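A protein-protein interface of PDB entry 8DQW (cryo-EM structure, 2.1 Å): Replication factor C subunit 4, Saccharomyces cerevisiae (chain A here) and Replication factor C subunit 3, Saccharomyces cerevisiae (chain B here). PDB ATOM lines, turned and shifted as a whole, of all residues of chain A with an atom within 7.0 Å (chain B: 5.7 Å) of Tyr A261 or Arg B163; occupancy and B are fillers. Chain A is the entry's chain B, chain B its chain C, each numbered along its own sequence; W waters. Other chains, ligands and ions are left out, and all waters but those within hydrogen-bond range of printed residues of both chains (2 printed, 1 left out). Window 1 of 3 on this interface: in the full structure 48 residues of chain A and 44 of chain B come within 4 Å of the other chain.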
ATOM      1  N   GLN A 204      16.457  28.783 -10.914  1.00  0.00           N
ATOM      2  CA  GLN A 204      16.582  27.456 -10.324  1.00  0.00           C
ATOM      3  C   GLN A 204      16.182  27.468  -8.855  1.00  0.00           C
ATOM      4  O   GLN A 204      15.577  26.509  -8.368  1.00  0.00           O
ATOM      5  CB  GLN A 204      18.012  26.940 -10.486  1.00  0.00           C
ATOM      6  CG  GLN A 204      18.311  26.346 -11.858  1.00  0.00           C
ATOM      7  CD  GLN A 204      17.445  25.142 -12.180  1.00  0.00           C
ATOM      8  OE1 GLN A 204      16.315  25.282 -12.647  1.00  0.00           O
ATOM      9  NE2 GLN A 204      17.973  23.949 -11.932  1.00  0.00           N
ATOM     10  N   ASN A 207      12.396  27.430  -8.791  1.00  0.00           N
ATOM     11  CA  ASN A 207      11.888  26.127  -9.210  1.00  0.00           C
ATOM     12  C   ASN A 207      12.081  25.082  -8.116  1.00  0.00           C
ATOM     13  O   ASN A 207      11.174  24.288  -7.839  1.00  0.00           O
ATOM     14  CB  ASN A 207      12.576  25.685 -10.503  1.00  0.00           C
ATOM     15  CG  ASN A 207      12.178  26.534 -11.695  1.00  0.00           C
ATOM     16  OD1 ASN A 207      11.309  27.398 -11.593  1.00  0.00           O
ATOM     17  ND2 ASN A 207      12.819  26.294 -12.832  1.00  0.00           N
ATOM     18  N   ASN A 208      13.254  25.070  -7.480  1.00  0.00           N
ATOM     19  CA  ASN A 208      13.513  24.097  -6.424  1.00  0.00           C
ATOM     20  C   ASN A 208      12.630  24.353  -5.209  1.00  0.00           C
ATOM     21  O   ASN A 208      12.138  23.406  -4.584  1.00  0.00           O
ATOM     22  CB  ASN A 208      14.990  24.128  -6.034  1.00  0.00           C
ATOM     23  CG  ASN A 208      15.879  23.469  -7.073  1.00  0.00           C
ATOM     24  OD1 ASN A 208      15.552  22.409  -7.606  1.00  0.00           O
ATOM     25  ND2 ASN A 208      17.014  24.093  -7.363  1.00  0.00           N
ATOM     26  N   SER A 211       9.210  23.037  -6.098  1.00  0.00           N
ATOM     27  CA  SER A 211       9.204  21.577  -6.089  1.00  0.00           C
ATOM     28  C   SER A 211       9.177  21.040  -4.664  1.00  0.00           C
ATOM     29  O   SER A 211       8.419  20.115  -4.350  1.00  0.00           O
ATOM     30  CB  SER A 211      10.425  21.046  -6.839  1.00  0.00           C
ATOM     31  OG  SER A 211      10.305  19.657  -7.086  1.00  0.00           O
ATOM     32  N   ILE A 227      14.856  15.901  -3.157  1.00  0.00           N
ATOM     33  CA  ILE A 227      14.549  16.199  -4.552  1.00  0.00           C
ATOM     34  C   ILE A 227      15.738  16.831  -5.262  1.00  0.00           C
ATOM     35  O   ILE A 227      16.144  16.381  -6.333  1.00  0.00           O
ATOM     36  CB  ILE A 227      13.303  17.111  -4.639  1.00  0.00           C
ATOM     37  CG1 ILE A 227      12.152  16.525  -3.814  1.00  0.00           C
ATOM     38  CG2 ILE A 227      12.895  17.315  -6.099  1.00  0.00           C
ATOM     39  CD1 ILE A 227      10.891  17.365  -3.831  1.00  0.00           C
ATOM     40  N   VAL A 228      16.308  17.876  -4.677  1.00  0.00           N
ATOM     41  CA  VAL A 228      17.392  18.629  -5.296  1.00  0.00           C
ATOM     42  C   VAL A 228      18.716  17.946  -4.988  1.00  0.00           C
ATOM     43  O   VAL A 228      18.918  17.408  -3.894  1.00  0.00           O
ATOM     44  CB  VAL A 228      17.393  20.089  -4.803  1.00  0.00           C
ATOM     45  CG1 VAL A 228      18.323  20.937  -5.654  1.00  0.00           C
ATOM     46  CG2 VAL A 228      15.981  20.657  -4.819  1.00  0.00           C
ATOM     47  N   ASP A 229      19.620  17.968  -5.962  1.00  0.00           N
ATOM     48  CA  ASP A 229      20.948  17.394  -5.830  1.00  0.00           C
ATOM     49  C   ASP A 229      21.986  18.508  -5.749  1.00  0.00           C
ATOM     50  O   ASP A 229      21.851  19.552  -6.394  1.00  0.00           O
ATOM     51  CB  ASP A 229      21.274  16.475  -7.011  1.00  0.00           C
ATOM     52  CG  ASP A 229      20.974  15.017  -6.717  1.00  0.00           C
ATOM     53  OD1 ASP A 229      19.921  14.736  -6.107  1.00  0.00           O
ATOM     54  OD2 ASP A 229      21.790  14.152  -7.099  1.00  0.00           O
ATOM     55  N   SER A 230      23.020  18.277  -4.952  1.00  0.00           N
ATOM     56  CA  SER A 230      24.110  19.235  -4.880  1.00  0.00           C
ATOM     57  C   SER A 230      24.753  19.376  -6.257  1.00  0.00           C
ATOM     58  O   SER A 230      24.852  18.389  -6.997  1.00  0.00           O
ATOM     59  CB  SER A 230      25.150  18.790  -3.852  1.00  0.00           C
ATOM     60  OG  SER A 230      26.365  19.499  -4.017  1.00  0.00           O
ATOM     61  N   PRO A 231      25.188  20.576  -6.642  1.00  0.00           N
ATOM     62  CA  PRO A 231      25.783  20.746  -7.978  1.00  0.00           C
ATOM     63  C   PRO A 231      26.956  19.799  -8.174  1.00  0.00           C
ATOM     64  O   PRO A 231      27.907  19.786  -7.389  1.00  0.00           O
ATOM     65  CB  PRO A 231      26.222  22.215  -7.990  1.00  0.00           C
ATOM     66  CG  PRO A 231      26.264  22.630  -6.558  1.00  0.00           C
ATOM     67  CD  PRO A 231      25.226  21.820  -5.857  1.00  0.00           C
ATOM     68  N   HIS A 232      26.882  18.999  -9.234  1.00  0.00           N
ATOM     69  CA  HIS A 232      27.890  17.977  -9.483  1.00  0.00           C
ATOM     70  C   HIS A 232      29.257  18.581  -9.806  1.00  0.00           C
ATOM     71  O   HIS A 232      30.269  17.892  -9.634  1.00  0.00           O
ATOM     72  CB  HIS A 232      27.431  17.020 -10.591  1.00  0.00           C
ATOM     73  CG  HIS A 232      27.464  17.603 -11.967  1.00  0.00           C
ATOM     74  ND1 HIS A 232      26.397  18.282 -12.515  1.00  0.00           N
ATOM     75  CD2 HIS A 232      28.427  17.586 -12.920  1.00  0.00           C
ATOM     76  CE1 HIS A 232      26.706  18.670 -13.738  1.00  0.00           C
ATOM     77  NE2 HIS A 232      27.931  18.260 -14.010  1.00  0.00           N
ATOM     78  N   ILE A 235      31.073  18.265  -6.623  1.00  0.00           N
ATOM     79  CA  ILE A 235      31.456  16.881  -6.366  1.00  0.00           C
ATOM     80  C   ILE A 235      32.683  16.514  -7.190  1.00  0.00           C
ATOM     81  O   ILE A 235      33.596  15.836  -6.706  1.00  0.00           O
ATOM     82  CB  ILE A 235      30.276  15.932  -6.658  1.00  0.00           C
ATOM     83  CG1 ILE A 235      29.064  16.296  -5.794  1.00  0.00           C
ATOM     84  CG2 ILE A 235      30.692  14.486  -6.431  1.00  0.00           C
ATOM     85  CD1 ILE A 235      29.134  15.762  -4.380  1.00  0.00           C
ATOM     86  N   ASP A 255      29.197   9.041  -5.327  1.00  0.00           N
ATOM     87  CA  ASP A 255      28.521  10.313  -5.546  1.00  0.00           C
ATOM     88  C   ASP A 255      28.159  10.574  -7.003  1.00  0.00           C
ATOM     89  O   ASP A 255      27.211  11.325  -7.260  1.00  0.00           O
ATOM     90  CB  ASP A 255      29.390  11.466  -5.032  1.00  0.00           C
ATOM     91  CG  ASP A 255      29.722  11.331  -3.556  1.00  0.00           C
ATOM     92  OD1 ASP A 255      28.990  10.616  -2.842  1.00  0.00           O
ATOM     93  OD2 ASP A 255      30.717  11.941  -3.110  1.00  0.00           O
ATOM     94  N   LEU A 256      28.884   9.992  -7.957  1.00  0.00           N
ATOM     95  CA  LEU A 256      28.636  10.248  -9.373  1.00  0.00           C
ATOM     96  C   LEU A 256      28.152   9.010 -10.115  1.00  0.00           C
ATOM     97  O   LEU A 256      27.077   9.047 -10.721  1.00  0.00           O
ATOM     98  CB  LEU A 256      29.904  10.807 -10.034  1.00  0.00           C
ATOM     99  CG  LEU A 256      30.518  12.043  -9.372  1.00  0.00           C
ATOM    100  CD1 LEU A 256      31.914  12.308  -9.914  1.00  0.00           C
ATOM    101  CD2 LEU A 256      29.623  13.252  -9.587  1.00  0.00           C
ATOM    102  N   TRP A 257      28.907   7.909 -10.086  1.00  0.00           N
ATOM    103  CA  TRP A 257      28.578   6.773 -10.940  1.00  0.00           C
ATOM    104  C   TRP A 257      27.257   6.131 -10.531  1.00  0.00           C
ATOM    105  O   TRP A 257      26.376   5.917 -11.372  1.00  0.00           O
ATOM    106  CB  TRP A 257      29.706   5.743 -10.905  1.00  0.00           C
ATOM    107  CG  TRP A 257      29.578   4.704 -11.975  1.00  0.00           C
ATOM    108  CD1 TRP A 257      29.269   3.387 -11.807  1.00  0.00           C
ATOM    109  CD2 TRP A 257      29.746   4.900 -13.385  1.00  0.00           C
ATOM    110  NE1 TRP A 257      29.238   2.749 -13.025  1.00  0.00           N
ATOM    111  CE2 TRP A 257      29.526   3.656 -14.008  1.00  0.00           C
ATOM    112  CE3 TRP A 257      30.061   6.006 -14.179  1.00  0.00           C
ATOM    113  CZ2 TRP A 257      29.615   3.488 -15.388  1.00  0.00           C
ATOM    114  CZ3 TRP A 257      30.149   5.837 -15.548  1.00  0.00           C
ATOM    115  CH2 TRP A 257      29.926   4.587 -16.139  1.00  0.00           C
ATOM    116  N   LYS A 258      27.096   5.820  -9.245  1.00  0.00           N
ATOM    117  CA  LYS A 258      25.889   5.144  -8.786  1.00  0.00           C
ATOM    118  C   LYS A 258      24.678   6.065  -8.712  1.00  0.00           C
ATOM    119  O   LYS A 258      23.571   5.577  -8.461  1.00  0.00           O
ATOM    120  CB  LYS A 258      26.125   4.495  -7.420  1.00  0.00           C
ATOM    121  CG  LYS A 258      26.977   3.235  -7.481  1.00  0.00           C
ATOM    122  CD  LYS A 258      27.347   2.739  -6.089  1.00  0.00           C
ATOM    123  CE  LYS A 258      28.435   1.667  -6.110  1.00  0.00           C
ATOM    124  NZ  LYS A 258      28.968   1.357  -7.468  1.00  0.00           N
ATOM    125  N   LYS A 259      24.853   7.367  -8.917  1.00  0.00           N
ATOM    126  CA  LYS A 259      23.734   8.295  -8.987  1.00  0.00           C
ATOM    127  C   LYS A 259      23.196   8.462 -10.402  1.00  0.00           C
ATOM    128  O   LYS A 259      22.234   9.209 -10.599  1.00  0.00           O
ATOM    129  CB  LYS A 259      24.144   9.661  -8.428  1.00  0.00           C
ATOM    130  CG  LYS A 259      24.365   9.666  -6.925  1.00  0.00           C
ATOM    131  CD  LYS A 259      23.832  10.938  -6.288  1.00  0.00           C
ATOM    132  CE  LYS A 259      24.187  11.011  -4.813  1.00  0.00           C
ATOM    133  NZ  LYS A 259      23.598   9.882  -4.042  1.00  0.00           N
ATOM    134  N   GLY A 260      23.789   7.790 -11.386  1.00  0.00           N
ATOM    135  CA  GLY A 260      23.306   7.843 -12.749  1.00  0.00           C
ATOM    136  C   GLY A 260      23.957   8.881 -13.633  1.00  0.00           C
ATOM    137  O   GLY A 260      23.450   9.136 -14.732  1.00  0.00           O
ATOM    138  N   TYR A 261      25.056   9.490 -13.199  1.00  0.00           N
ATOM    139  CA  TYR A 261      25.740  10.470 -14.031  1.00  0.00           C
ATOM    140  C   TYR A 261      26.515   9.766 -15.139  1.00  0.00           C
ATOM    141  O   TYR A 261      27.247   8.804 -14.885  1.00  0.00           O
ATOM    142  CB  TYR A 261      26.678  11.321 -13.177  1.00  0.00           C
ATOM    143  CG  TYR A 261      25.952  12.360 -12.358  1.00  0.00           C
ATOM    144  CD1 TYR A 261      25.490  13.531 -12.940  1.00  0.00           C
ATOM    145  CD2 TYR A 261      25.713  12.162 -11.005  1.00  0.00           C
ATOM    146  CE1 TYR A 261      24.819  14.482 -12.197  1.00  0.00           C
ATOM    147  CE2 TYR A 261      25.043  13.106 -10.254  1.00  0.00           C
ATOM    148  CZ  TYR A 261      24.597  14.264 -10.855  1.00  0.00           C
ATOM    149  OH  TYR A 261      23.930  15.208 -10.112  1.00  0.00           O
ATOM    150  N   SER A 262      26.349  10.242 -16.370  1.00  0.00           N
ATOM    151  CA  SER A 262      27.029   9.636 -17.505  1.00  0.00           C
ATOM    152  C   SER A 262      28.517   9.973 -17.484  1.00  0.00           C
ATOM    153  O   SER A 262      28.938  11.006 -16.958  1.00  0.00           O
ATOM    154  CB  SER A 262      26.404  10.111 -18.817  1.00  0.00           C
ATOM    155  OG  SER A 262      26.541  11.511 -18.971  1.00  0.00           O
ATOM    156  N   SER A 263      29.319   9.081 -18.072  1.00  0.00           N
ATOM    157  CA  SER A 263      30.765   9.280 -18.079  1.00  0.00           C
ATOM    158  C   SER A 263      31.150  10.536 -18.853  1.00  0.00           C
ATOM    159  O   SER A 263      32.058  11.272 -18.445  1.00  0.00           O
ATOM    160  CB  SER A 263      31.458   8.048 -18.665  1.00  0.00           C
ATOM    161  OG  SER A 263      31.108   7.859 -20.024  1.00  0.00           O
ATOM    162  N   ILE A 264      30.472  10.798 -19.973  1.00  0.00           N
ATOM    163  CA  ILE A 264      30.793  11.973 -20.780  1.00  0.00           C
ATOM    164  C   ILE A 264      30.574  13.249 -19.974  1.00  0.00           C
ATOM    165  O   ILE A 264      31.403  14.172 -19.998  1.00  0.00           O
ATOM    166  CB  ILE A 264      29.970  11.969 -22.085  1.00  0.00           C
ATOM    167  CG1 ILE A 264      30.382  13.133 -22.991  1.00  0.00           C
ATOM    168  CG2 ILE A 264      28.474  12.039 -21.790  1.00  0.00           C
ATOM    169  CD1 ILE A 264      31.749  12.970 -23.610  1.00  0.00           C
ATOM    170  N   ASP A 265      29.457  13.325 -19.246  1.00  0.00           N
ATOM    171  CA  ASP A 265      29.209  14.485 -18.398  1.00  0.00           C
ATOM    172  C   ASP A 265      30.297  14.626 -17.343  1.00  0.00           C
ATOM    173  O   ASP A 265      30.771  15.737 -17.070  1.00  0.00           O
ATOM    174  CB  ASP A 265      27.834  14.368 -17.732  1.00  0.00           C
ATOM    175  CG  ASP A 265      26.689  14.645 -18.691  1.00  0.00           C
ATOM    176  OD1 ASP A 265      26.871  15.449 -19.629  1.00  0.00           O
ATOM    177  OD2 ASP A 265      25.602  14.059 -18.505  1.00  0.00           O
ATOM    178  N   ILE A 266      30.716  13.507 -16.750  1.00  0.00           N
ATOM    179  CA  ILE A 266      31.737  13.549 -15.707  1.00  0.00           C
ATOM    180  C   ILE A 266      33.040  14.116 -16.262  1.00  0.00           C
ATOM    181  O   ILE A 266      33.675  14.972 -15.639  1.00  0.00           O
ATOM    182  CB  ILE A 266      31.941  12.148 -15.103  1.00  0.00           C
ATOM    183  CG1 ILE A 266      30.692  11.728 -14.323  1.00  0.00           C
ATOM    184  CG2 ILE A 266      33.181  12.126 -14.208  1.00  0.00           C
ATOM    185  CD1 ILE A 266      30.730  10.306 -13.807  1.00  0.00           C
ATOM    186  N   LEU A 309      37.354   5.927 -16.217  1.00  0.00           N
ATOM    187  CA  LEU A 309      37.382   7.049 -15.283  1.00  0.00           C
ATOM    188  C   LEU A 309      38.299   6.763 -14.100  1.00  0.00           C
ATOM    189  O   LEU A 309      39.017   7.656 -13.631  1.00  0.00           O
ATOM    190  CB  LEU A 309      35.965   7.364 -14.801  1.00  0.00           C
ATOM    191  CG  LEU A 309      34.990   7.839 -15.881  1.00  0.00           C
ATOM    192  CD1 LEU A 309      33.561   7.847 -15.356  1.00  0.00           C
ATOM    193  CD2 LEU A 309      35.381   9.214 -16.395  1.00  0.00           C
ATOM    194  N   HIS B  48       7.695  23.228 -15.895  1.00  0.00           N
ATOM    195  CA  HIS B  48       8.519  22.633 -16.940  1.00  0.00           C
ATOM    196  C   HIS B  48       9.475  21.623 -16.316  1.00  0.00           C
ATOM    197  O   HIS B  48      10.109  21.900 -15.294  1.00  0.00           O
ATOM    198  CB  HIS B  48       9.288  23.719 -17.691  1.00  0.00           C
ATOM    199  CG  HIS B  48       8.418  24.815 -18.220  1.00  0.00           C
ATOM    200  ND1 HIS B  48       7.542  24.630 -19.268  1.00  0.00           N
ATOM    201  CD2 HIS B  48       8.284  26.108 -17.843  1.00  0.00           C
ATOM    202  CE1 HIS B  48       6.906  25.761 -19.514  1.00  0.00           C
ATOM    203  NE2 HIS B  48       7.339  26.675 -18.663  1.00  0.00           N
ATOM    204  N   LEU B  50      12.484  18.435 -16.419  1.00  0.00           N
ATOM    205  CA  LEU B  50      13.636  17.765 -17.004  1.00  0.00           C
ATOM    206  C   LEU B  50      13.800  16.426 -16.305  1.00  0.00           C
ATOM    207  O   LEU B  50      13.864  16.373 -15.074  1.00  0.00           O
ATOM    208  CB  LEU B  50      14.912  18.608 -16.864  1.00  0.00           C
ATOM    209  CG  LEU B  50      16.249  17.874 -17.040  1.00  0.00           C
ATOM    210  CD1 LEU B  50      16.382  17.325 -18.449  1.00  0.00           C
ATOM    211  CD2 LEU B  50      17.417  18.794 -16.717  1.00  0.00           C
ATOM    212  N   TYR B  52      16.431  13.535 -16.166  1.00  0.00           N
ATOM    213  CA  TYR B  52      17.807  13.195 -16.502  1.00  0.00           C
ATOM    214  C   TYR B  52      18.154  11.840 -15.907  1.00  0.00           C
ATOM    215  O   TYR B  52      17.957  11.621 -14.707  1.00  0.00           O
ATOM    216  CB  TYR B  52      18.776  14.260 -15.982  1.00  0.00           C
ATOM    217  CG  TYR B  52      20.230  13.878 -16.134  1.00  0.00           C
ATOM    218  CD1 TYR B  52      20.859  13.940 -17.371  1.00  0.00           C
ATOM    219  CD2 TYR B  52      20.973  13.449 -15.042  1.00  0.00           C
ATOM    220  CE1 TYR B  52      22.188  13.590 -17.516  1.00  0.00           C
ATOM    221  CE2 TYR B  52      22.304  13.096 -15.177  1.00  0.00           C
ATOM    222  CZ  TYR B  52      22.906  13.169 -16.416  1.00  0.00           C
ATOM    223  OH  TYR B  52      24.230  12.820 -16.556  1.00  0.00           O
ATOM    224  N   PRO B  54      20.187   7.568 -16.773  1.00  0.00           N
ATOM    225  CA  PRO B  54      20.810   6.588 -17.671  1.00  0.00           C
ATOM    226  C   PRO B  54      19.768   5.717 -18.349  1.00  0.00           C
ATOM    227  O   PRO B  54      18.580   5.763 -17.999  1.00  0.00           O
ATOM    228  CB  PRO B  54      21.706   5.762 -16.735  1.00  0.00           C
ATOM    229  CG  PRO B  54      21.189   5.997 -15.349  1.00  0.00           C
ATOM    230  CD  PRO B  54      20.208   7.134 -15.366  1.00  0.00           C
ATOM    231  N   LEU B 158      18.605  24.433 -19.341  1.00  0.00           N
ATOM    232  CA  LEU B 158      18.681  23.800 -18.029  1.00  0.00           C
ATOM    233  C   LEU B 158      18.118  24.712 -16.945  1.00  0.00           C
ATOM    234  O   LEU B 158      17.450  24.245 -16.015  1.00  0.00           O
ATOM    235  CB  LEU B 158      20.128  23.422 -17.710  1.00  0.00           C
ATOM    236  CG  LEU B 158      20.663  22.166 -18.402  1.00  0.00           C
ATOM    237  CD1 LEU B 158      22.180  22.210 -18.496  1.00  0.00           C
ATOM    238  CD2 LEU B 158      20.207  20.915 -17.675  1.00  0.00           C
ATOM    239  N   CYS B 161      14.125  24.535 -16.522  1.00  0.00           N
ATOM    240  CA  CYS B 161      13.445  23.282 -16.226  1.00  0.00           C
ATOM    241  C   CYS B 161      13.686  22.862 -14.783  1.00  0.00           C
ATOM    242  O   CYS B 161      14.800  22.994 -14.265  1.00  0.00           O
ATOM    243  CB  CYS B 161      13.920  22.171 -17.167  1.00  0.00           C
ATOM    244  SG  CYS B 161      13.536  22.455 -18.912  1.00  0.00           S
ATOM    245  N   THR B 162      12.635  22.354 -14.141  1.00  0.00           N
ATOM    246  CA  THR B 162      12.761  21.713 -12.838  1.00  0.00           C
ATOM    247  C   THR B 162      13.341  20.318 -13.040  1.00  0.00           C
ATOM    248  O   THR B 162      12.764  19.504 -13.766  1.00  0.00           O
ATOM    249  CB  THR B 162      11.405  21.637 -12.142  1.00  0.00           C
ATOM    250  OG1 THR B 162      10.819  22.943 -12.077  1.00  0.00           O
ATOM    251  CG2 THR B 162      11.553  21.075 -10.736  1.00  0.00           C
ATOM    252  N   ARG B 163      14.471  20.040 -12.397  1.00  0.00           N
ATOM    253  CA  ARG B 163      15.285  18.874 -12.710  1.00  0.00           C
ATOM    254  C   ARG B 163      14.943  17.714 -11.784  1.00  0.00           C
ATOM    255  O   ARG B 163      14.845  17.892 -10.565  1.00  0.00           O
ATOM    256  CB  ARG B 163      16.771  19.223 -12.596  1.00  0.00           C
ATOM    257  CG  ARG B 163      17.698  18.033 -12.408  1.00  0.00           C
ATOM    258  CD  ARG B 163      19.071  18.319 -13.002  1.00  0.00           C
ATOM    259  NE  ARG B 163      19.953  17.157 -12.980  1.00  0.00           N
ATOM    260  CZ  ARG B 163      20.403  16.574 -11.878  1.00  0.00           C
ATOM    261  NH1 ARG B 163      20.092  17.029 -10.675  1.00  0.00           N
ATOM    262  NH2 ARG B 163      21.192  15.509 -11.985  1.00  0.00           N
ATOM    263  N   PHE B 164      14.771  16.528 -12.367  1.00  0.00           N
ATOM    264  CA  PHE B 164      14.545  15.295 -11.629  1.00  0.00           C
ATOM    265  C   PHE B 164      15.496  14.233 -12.157  1.00  0.00           C
ATOM    266  O   PHE B 164      15.560  13.996 -13.372  1.00  0.00           O
ATOM    267  CB  PHE B 164      13.092  14.822 -11.761  1.00  0.00           C
ATOM    268  CG  PHE B 164      12.103  15.692 -11.040  1.00  0.00           C
ATOM    269  CD1 PHE B 164      11.878  15.529  -9.684  1.00  0.00           C
ATOM    270  CD2 PHE B 164      11.398  16.672 -11.718  1.00  0.00           C
ATOM    271  CE1 PHE B 164      10.968  16.328  -9.017  1.00  0.00           C
ATOM    272  CE2 PHE B 164      10.488  17.474 -11.055  1.00  0.00           C
ATOM    273  CZ  PHE B 164      10.272  17.301  -9.703  1.00  0.00           C
ATOM    274  N   ARG B 165      16.217  13.591 -11.244  1.00  0.00           N
ATOM    275  CA  ARG B 165      17.225  12.597 -11.584  1.00  0.00           C
ATOM    276  C   ARG B 165      16.649  11.203 -11.376  1.00  0.00           C
ATOM    277  O   ARG B 165      16.185  10.875 -10.278  1.00  0.00           O
ATOM    278  CB  ARG B 165      18.480  12.789 -10.733  1.00  0.00           C
ATOM    279  CG  ARG B 165      19.661  11.935 -11.167  1.00  0.00           C
ATOM    280  CD  ARG B 165      20.907  12.244 -10.349  1.00  0.00           C
ATOM    281  NE  ARG B 165      20.618  12.349  -8.923  1.00  0.00           N
ATOM    282  CZ  ARG B 165      20.427  11.313  -8.116  1.00  0.00           C
ATOM    283  NH1 ARG B 165      20.496  10.069  -8.560  1.00  0.00           N
ATOM    284  NH2 ARG B 165      20.159  11.532  -6.832  1.00  0.00           N
HETATM  285  O   HOH W   1      10.338  24.594 -14.400  1.00  0.00           O
HETATM  286  O   HOH W   2       9.391  23.890  -9.772  1.00  0.00           O
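NH1 of Arg B165 lies within hydrogen-bond range of O of Lys A259, 2.8 Å away. OE1 of Gln A204 lies close to O of Cys B161 (3.2 Å). The side-chain hydroxyl (OH) of Tyr A261 lies within hydrogen-bond range of the guanidinium group (NH2) of Arg B163, at 3.3 Å. OD2 of Asp A265 lies within hydrogen-bond range of OH of Tyr B52, at 2.7 Å. The backbone NH (N) of Ser A262 lies within hydrogen-bond range of the side-chain hydroxyl (OH) of Tyr B52, at 3.3 Å. OD2 of Asp A229 lies within salt-bridge range of NE of Arg B165 (2.8 Å).
Of the printed residues of chain B, Gln A204 touches Leu B158 (3.7 Å) and Cys B161 (3.2 Å). Printed residues of chain B within 4 Å of Gly A260: Pro B54 (3.8 Å). Tyr A261 touches two residues of chain B. Arg B163 touches just these residues of chain A: Asp A229 and Tyr A261.
The backbone carbonyl oxygen of His B48 lies within hydrogen-bond range of the backbone NH of Thr B162. OG of Ser A262 lies within hydrogen-bond range of OD2 of Asp A265 (2.8 Å). O of Leu B50 is in hydrogen-bond range of N of Phe B164 (2.9 Å). The backbone carbonyl oxygen (O) of Phe B164 sits at hydrogen-bond distance from the backbone NH (N) of Tyr B52 (3.0 Å). The side-chain amide nitrogen (ND2) of Asn A208 sits at hydrogen-bond distance from the backbone carbonyl oxygen (O) of Gln A204 (3.0 Å). N of Leu B50 lies within hydrogen-bond range of O of Thr B162 (2.9 Å).
Water W2 lies within hydrogen-bond range of O of Asn A207 (2.7 Å) and OG1 of Thr B162 (2.9 Å). Water W1 lies within hydrogen-bond range of O of His B48, OG1 of Thr B162 and ND2 of Asn A207.
Among the printed residues, merely in contact across the chains: Ser A211 with Phe B164, Asn A207 with Thr B162, Ile A227 with Phe B164, Gln A204 with Leu B158, Tyr A261 with Tyr B52, Gly A260 with Pro B54 and Asp A229 with Arg B163.
Printed residues of chain B that touch a printed residue of chain A: Tyr B52, Pro B54, Leu B158, Cys B161, Thr B162, Arg B163, Phe B164 and Arg B165. Among the printed residues, Asp or Glu carboxylates within 4 Å of a Lys or Arg side-chain nitrogen of the other chain: Asp A229 with Arg B165 (2.8 Å).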
